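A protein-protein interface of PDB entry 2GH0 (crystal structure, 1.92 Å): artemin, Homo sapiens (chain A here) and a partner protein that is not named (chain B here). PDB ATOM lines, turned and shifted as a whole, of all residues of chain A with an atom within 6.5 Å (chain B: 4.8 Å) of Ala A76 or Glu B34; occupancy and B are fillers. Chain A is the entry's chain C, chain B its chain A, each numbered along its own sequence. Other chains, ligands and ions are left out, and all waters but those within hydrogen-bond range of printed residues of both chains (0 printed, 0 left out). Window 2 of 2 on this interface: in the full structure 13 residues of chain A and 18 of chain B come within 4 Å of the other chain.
Among the printed residues, pairs that only touch across the chains: Ala A76 with Glu B34, Ser A78 with Lys B30, Ser A78 with Glu B34, Trp A86 with Tyr B32, Trp A86 with Gly B33, Trp A86 with Ser B37, Arg A87 with Ser B37, Thr A88 with Gly B33 and Thr A88 with Glu B34.
Hydrophobic or aromatic side chains of chain A that line the printed part of chain B: Ala A76 and Trp A86. Along chain A the printed residues that touch a printed residue of chain B span positions 76 to 88. Among the printed residues, 10 pairs touch across the chains. Among the printed residues, no Asp or Glu carboxylate lies within 4 Å of a Lys or Arg side-chain nitrogen of the other chain.
OG1 of Thr A88 is in hydrogen-bond range of OG of Ser B37 (2.7 Å).
Ala A76 touches just one residue of chain B: Glu B34. Val A89 touches none of the printed residues of chain B. Of the printed residues of chain A, Lys B30 touches Ser A78. Glu B34 touches three residues of chain A. Cys B36 touches none of the printed residues of chain A. Printed residues of chain A within 4 Å of Ser B37: Trp A86 (3.8 Å), Arg A87 (3.8 Å) and Thr A88 (2.7 Å). The nearest residue of chain B that does not touch Ala A76 is Lys B30 (4.6 Å). The nearest residue of chain A that does not touch Glu B34 is Asp A90 (4.9 Å). The nearest printed residue of chain A that does not touch Ser B37 is Ser A78 (4.9 Å).
OG of Ser A78 lies within hydrogen-bond range of OG1 of Thr A88 (3.1 Å). The side-chain hydroxyl (OG) of Ser B37 sits at hydrogen-bond distance from the backbone carbonyl oxygen (O) of Gly B33.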
ATOM      1  N   TYR A  74       9.967   8.003 -15.503  1.00  0.00           N
ATOM      2  CA  TYR A  74       9.349   8.569 -16.707  1.00  0.00           C
ATOM      3  C   TYR A  74       7.826   8.257 -16.772  1.00  0.00           C
ATOM      4  O   TYR A  74       7.320   7.338 -16.097  1.00  0.00           O
ATOM      5  CB  TYR A  74      10.017   7.966 -17.961  1.00  0.00           C
ATOM      6  CG  TYR A  74      11.528   8.172 -18.120  1.00  0.00           C
ATOM      7  CD1 TYR A  74      12.025   9.234 -18.869  1.00  0.00           C
ATOM      8  CD2 TYR A  74      12.447   7.280 -17.536  1.00  0.00           C
ATOM      9  CE1 TYR A  74      13.442   9.424 -19.025  1.00  0.00           C
ATOM     10  CE2 TYR A  74      13.843   7.458 -17.674  1.00  0.00           C
ATOM     11  CZ  TYR A  74      14.339   8.520 -18.449  1.00  0.00           C
ATOM     12  OH  TYR A  74      15.740   8.751 -18.616  1.00  0.00           O
ATOM     13  N   GLU A  75       7.117   9.010 -17.591  1.00  0.00           N
ATOM     14  CA  GLU A  75       5.708   8.677 -17.924  1.00  0.00           C
ATOM     15  C   GLU A  75       5.481   8.917 -19.413  1.00  0.00           C
ATOM     16  O   GLU A  75       6.305   9.591 -20.083  1.00  0.00           O
ATOM     17  CB  GLU A  75       4.724   9.514 -17.097  1.00  0.00           C
ATOM     18  CG  GLU A  75       4.850  11.063 -17.351  1.00  0.00           C
ATOM     19  CD  GLU A  75       3.804  11.874 -16.594  1.00  0.00           C
ATOM     20  OE1 GLU A  75       2.820  11.273 -16.057  1.00  0.00           O
ATOM     21  OE2 GLU A  75       3.948  13.126 -16.540  1.00  0.00           O
ATOM     22  N   ALA A  76       4.332   8.440 -19.918  1.00  0.00           N
ATOM     23  CA  ALA A  76       4.047   8.586 -21.331  1.00  0.00           C
ATOM     24  C   ALA A  76       3.572  10.004 -21.630  1.00  0.00           C
ATOM     25  O   ALA A  76       3.139  10.727 -20.739  1.00  0.00           O
ATOM     26  CB  ALA A  76       2.984   7.581 -21.769  1.00  0.00           C
ATOM     27  N   VAL A  77       3.625  10.366 -22.902  1.00  0.00           N
ATOM     28  CA  VAL A  77       2.957  11.559 -23.422  1.00  0.00           C
ATOM     29  C   VAL A  77       1.858  11.113 -24.427  1.00  0.00           C
ATOM     30  O   VAL A  77       2.091  10.229 -25.266  1.00  0.00           O
ATOM     31  CB  VAL A  77       3.986  12.417 -24.116  1.00  0.00           C
ATOM     32  CG1 VAL A  77       3.349  13.436 -24.990  1.00  0.00           C
ATOM     33  CG2 VAL A  77       4.941  13.061 -23.039  1.00  0.00           C
ATOM     34  N   SER A  78       0.687  11.749 -24.370  1.00  0.00           N
ATOM     35  CA  SER A  78      -0.484  11.341 -25.205  1.00  0.00           C
ATOM     36  C   SER A  78      -1.045  12.578 -25.837  1.00  0.00           C
ATOM     37  O   SER A  78      -1.049  13.645 -25.205  1.00  0.00           O
ATOM     38  CB  SER A  78      -1.591  10.745 -24.363  1.00  0.00           C
ATOM     39  OG  SER A  78      -1.101   9.618 -23.625  1.00  0.00           O
ATOM     40  N   TRP A  86      -5.980   9.167 -31.269  1.00  0.00           N
ATOM     41  CA  TRP A  86      -5.139   9.205 -30.057  1.00  0.00           C
ATOM     42  C   TRP A  86      -3.894   8.324 -30.178  1.00  0.00           C
ATOM     43  O   TRP A  86      -3.982   7.135 -30.509  1.00  0.00           O
ATOM     44  CB  TRP A  86      -5.932   8.720 -28.849  1.00  0.00           C
ATOM     45  CG  TRP A  86      -6.825   9.759 -28.259  1.00  0.00           C
ATOM     46  CD1 TRP A  86      -8.162   9.938 -28.471  1.00  0.00           C
ATOM     47  CD2 TRP A  86      -6.417  10.764 -27.324  1.00  0.00           C
ATOM     48  NE1 TRP A  86      -8.609  11.019 -27.707  1.00  0.00           N
ATOM     49  CE2 TRP A  86      -7.554  11.542 -27.005  1.00  0.00           C
ATOM     50  CE3 TRP A  86      -5.197  11.090 -26.743  1.00  0.00           C
ATOM     51  CZ2 TRP A  86      -7.493  12.618 -26.086  1.00  0.00           C
ATOM     52  CZ3 TRP A  86      -5.123  12.191 -25.861  1.00  0.00           C
ATOM     53  CH2 TRP A  86      -6.285  12.926 -25.551  1.00  0.00           C
ATOM     54  N   ARG A  87      -2.748   8.917 -29.813  1.00  0.00           N
ATOM     55  CA  ARG A  87      -1.461   8.264 -29.827  1.00  0.00           C
ATOM     56  C   ARG A  87      -0.820   8.444 -28.446  1.00  0.00           C
ATOM     57  O   ARG A  87      -1.039   9.457 -27.761  1.00  0.00           O
ATOM     58  CB  ARG A  87      -0.548   8.882 -30.891  1.00  0.00           C
ATOM     59  CG  ARG A  87      -1.112   8.893 -32.314  1.00  0.00           C
ATOM     60  CD  ARG A  87      -1.315   7.478 -32.899  1.00  0.00           C
ATOM     61  NE  ARG A  87      -1.828   7.480 -34.276  1.00  0.00           N
ATOM     62  CZ  ARG A  87      -2.141   6.379 -34.946  1.00  0.00           C
ATOM     63  NH1 ARG A  87      -2.003   5.198 -34.362  1.00  0.00           N
ATOM     64  NH2 ARG A  87      -2.602   6.445 -36.201  1.00  0.00           N
ATOM     65  N   THR A  88      -0.021   7.461 -28.043  1.00  0.00           N
ATOM     66  CA  THR A  88       0.740   7.533 -26.792  1.00  0.00           C
ATOM     67  C   THR A  88       2.135   6.991 -27.057  1.00  0.00           C
ATOM     68  O   THR A  88       2.295   5.942 -27.684  1.00  0.00           O
ATOM     69  CB  THR A  88       0.090   6.712 -25.668  1.00  0.00           C
ATOM     70  OG1 THR A  88      -1.244   7.170 -25.490  1.00  0.00           O
ATOM     71  CG2 THR A  88       0.787   6.959 -24.346  1.00  0.00           C
ATOM     72  N   VAL A  89       3.111   7.736 -26.583  1.00  0.00           N
ATOM     73  CA  VAL A  89       4.522   7.352 -26.637  1.00  0.00           C
ATOM     74  C   VAL A  89       5.022   7.206 -25.204  1.00  0.00           C
ATOM     75  O   VAL A  89       5.066   8.195 -24.445  1.00  0.00           O
ATOM     76  CB  VAL A  89       5.363   8.415 -27.370  1.00  0.00           C
ATOM     77  CG1 VAL A  89       6.874   7.967 -27.422  1.00  0.00           C
ATOM     78  CG2 VAL A  89       4.791   8.709 -28.753  1.00  0.00           C
ATOM     79  N   ASP A  90       5.451   5.990 -24.863  1.00  0.00           N
ATOM     80  CA  ASP A  90       5.832   5.638 -23.503  1.00  0.00           C
ATOM     81  C   ASP A  90       7.192   6.268 -23.108  1.00  0.00           C
ATOM     82  O   ASP A  90       8.031   6.533 -23.978  1.00  0.00           O
ATOM     83  CB  ASP A  90       5.956   4.124 -23.365  1.00  0.00           C
ATOM     84  CG  ASP A  90       4.667   3.385 -23.686  1.00  0.00           C
ATOM     85  OD1 ASP A  90       3.563   3.979 -23.556  1.00  0.00           O
ATOM     86  OD2 ASP A  90       4.778   2.187 -24.047  1.00  0.00           O
ATOM     87  N   ARG A  91       7.390   6.480 -21.809  1.00  0.00           N
ATOM     88  CA  ARG A  91       8.675   6.902 -21.236  1.00  0.00           C
ATOM     89  C   ARG A  91       9.290   8.152 -21.896  1.00  0.00           C
ATOM     90  O   ARG A  91      10.520   8.287 -21.973  1.00  0.00           O
ATOM     91  CB  ARG A  91       9.703   5.745 -21.205  1.00  0.00           C
ATOM     92  CG  ARG A  91       9.196   4.385 -20.571  1.00  0.00           C
ATOM     93  CD  ARG A  91      10.353   3.346 -20.548  1.00  0.00           C
ATOM     94  NE  ARG A  91       9.980   1.986 -20.131  1.00  0.00           N
ATOM     95  CZ  ARG A  91      10.867   0.996 -19.948  1.00  0.00           C
ATOM     96  NH1 ARG A  91      12.176   1.228 -20.122  1.00  0.00           N
ATOM     97  NH2 ARG A  91      10.470  -0.219 -19.571  1.00  0.00           N
ATOM     98  N   LEU A  92       8.437   9.059 -22.376  1.00  0.00           N
ATOM     99  CA  LEU A  92       8.887  10.261 -23.107  1.00  0.00           C
ATOM    100  C   LEU A  92       9.245  11.409 -22.187  1.00  0.00           C
ATOM    101  O   LEU A  92      10.155  12.197 -22.518  1.00  0.00           O
ATOM    102  CB  LEU A  92       7.827  10.740 -24.122  1.00  0.00           C
ATOM    103  CG  LEU A  92       8.302  11.378 -25.445  1.00  0.00           C
ATOM    104  CD1 LEU A  92       7.181  11.982 -26.198  1.00  0.00           C
ATOM    105  CD2 LEU A  92       9.317  12.442 -25.268  1.00  0.00           C
ATOM    106  N   SER A  93       8.551  11.520 -21.051  1.00  0.00           N
ATOM    107  CA  SER A  93       8.633  12.737 -20.180  1.00  0.00           C
ATOM    108  C   SER A  93       9.072  12.322 -18.778  1.00  0.00           C
ATOM    109  O   SER A  93       8.651  11.268 -18.293  1.00  0.00           O
ATOM    110  CB  SER A  93       7.249  13.466 -20.123  1.00  0.00           C
ATOM    111  OG  SER A  93       7.300  14.694 -19.397  1.00  0.00           O
ATOM    112  N   LYS B  30      -4.778  13.509 -20.119  1.00  0.00           N
ATOM    113  CA  LYS B  30      -3.643  12.639 -20.437  1.00  0.00           C
ATOM    114  C   LYS B  30      -3.915  11.198 -19.974  1.00  0.00           C
ATOM    115  O   LYS B  30      -3.513  10.235 -20.645  1.00  0.00           O
ATOM    116  CB  LYS B  30      -2.339  13.158 -19.783  1.00  0.00           C
ATOM    117  CG  LYS B  30      -1.574  14.157 -20.706  1.00  0.00           C
ATOM    118  CD  LYS B  30      -0.038  14.125 -20.470  1.00  0.00           C
ATOM    119  CE  LYS B  30       0.819  14.620 -21.676  1.00  0.00           C
ATOM    120  NZ  LYS B  30       2.207  15.354 -21.064  1.00  0.00           N
ATOM    121  N   ALA B  31      -4.505  11.071 -18.785  1.00  0.00           N
ATOM    122  CA  ALA B  31      -4.852   9.780 -18.221  1.00  0.00           C
ATOM    123  C   ALA B  31      -5.809   8.965 -19.107  1.00  0.00           C
ATOM    124  O   ALA B  31      -5.547   7.787 -19.352  1.00  0.00           O
ATOM    125  CB  ALA B  31      -5.447   9.949 -16.815  1.00  0.00           C
ATOM    126  N   TYR B  32      -6.910   9.563 -19.600  1.00  0.00           N
ATOM    127  CA  TYR B  32      -7.788   8.767 -20.449  1.00  0.00           C
ATOM    128  C   TYR B  32      -7.224   8.610 -21.850  1.00  0.00           C
ATOM    129  O   TYR B  32      -7.472   7.599 -22.505  1.00  0.00           O
ATOM    130  CB  TYR B  32      -9.252   9.282 -20.472  1.00  0.00           C
ATOM    131  CG  TYR B  32      -9.597  10.410 -21.469  1.00  0.00           C
ATOM    132  CD1 TYR B  32      -9.864  11.706 -21.031  1.00  0.00           C
ATOM    133  CD2 TYR B  32      -9.685  10.152 -22.851  1.00  0.00           C
ATOM    134  CE1 TYR B  32     -10.206  12.719 -21.949  1.00  0.00           C
ATOM    135  CE2 TYR B  32     -10.025  11.119 -23.758  1.00  0.00           C
ATOM    136  CZ  TYR B  32     -10.291  12.411 -23.307  1.00  0.00           C
ATOM    137  OH  TYR B  32     -10.619  13.410 -24.226  1.00  0.00           O
ATOM    138  N   GLY B  33      -6.491   9.623 -22.325  1.00  0.00           N
ATOM    139  CA  GLY B  33      -5.886   9.526 -23.640  1.00  0.00           C
ATOM    140  C   GLY B  33      -4.952   8.331 -23.687  1.00  0.00           C
ATOM    141  O   GLY B  33      -4.888   7.624 -24.697  1.00  0.00           O
ATOM    142  N   GLU B  34      -4.194   8.134 -22.603  1.00  0.00           N
ATOM    143  CA  GLU B  34      -3.302   6.970 -22.479  1.00  0.00           C
ATOM    144  C   GLU B  34      -4.077   5.648 -22.416  1.00  0.00           C
ATOM    145  O   GLU B  34      -3.681   4.665 -23.072  1.00  0.00           O
ATOM    146  CB  GLU B  34      -2.413   7.075 -21.232  1.00  0.00           C
ATOM    147  CG  GLU B  34      -1.453   5.901 -21.057  1.00  0.00           C
ATOM    148  CD  GLU B  34      -0.421   6.118 -19.963  1.00  0.00           C
ATOM    149  OE1 GLU B  34      -0.585   7.038 -19.126  1.00  0.00           O
ATOM    150  OE2 GLU B  34       0.558   5.331 -19.925  1.00  0.00           O
ATOM    151  N   ALA B  35      -5.096   5.615 -21.570  1.00  0.00           N
ATOM    152  CA  ALA B  35      -5.968   4.422 -21.382  1.00  0.00           C
ATOM    153  C   ALA B  35      -6.765   4.019 -22.641  1.00  0.00           C
ATOM    154  O   ALA B  35      -7.079   2.861 -22.831  1.00  0.00           O
ATOM    155  CB  ALA B  35      -6.886   4.624 -20.212  1.00  0.00           C
ATOM    156  N   CYS B  36      -6.989   4.975 -23.529  1.00  0.00           N
ATOM    157  CA  CYS B  36      -7.863   4.808 -24.655  1.00  0.00           C
ATOM    158  C   CYS B  36      -7.134   4.733 -25.997  1.00  0.00           C
ATOM    159  O   CYS B  36      -7.785   4.606 -27.036  1.00  0.00           O
ATOM    160  CB  CYS B  36      -8.873   5.942 -24.681  1.00  0.00           C
ATOM    161  SG  CYS B  36      -9.944   6.083 -23.234  1.00  0.00           S
ATOM    162  N   SER B  37      -5.803   4.800 -25.976  1.00  0.00           N
ATOM    163  CA  SER B  37      -4.970   4.722 -27.176  1.00  0.00           C
ATOM    164  C   SER B  37      -4.728   3.301 -27.703  1.00  0.00           C
ATOM    165  O   SER B  37      -4.601   2.328 -26.941  1.00  0.00           O
ATOM    166  CB  SER B  37      -3.555   5.311 -26.896  1.00  0.00           C
ATOM    167  OG  SER B  37      -3.657   6.689 -26.613  1.00  0.00           O
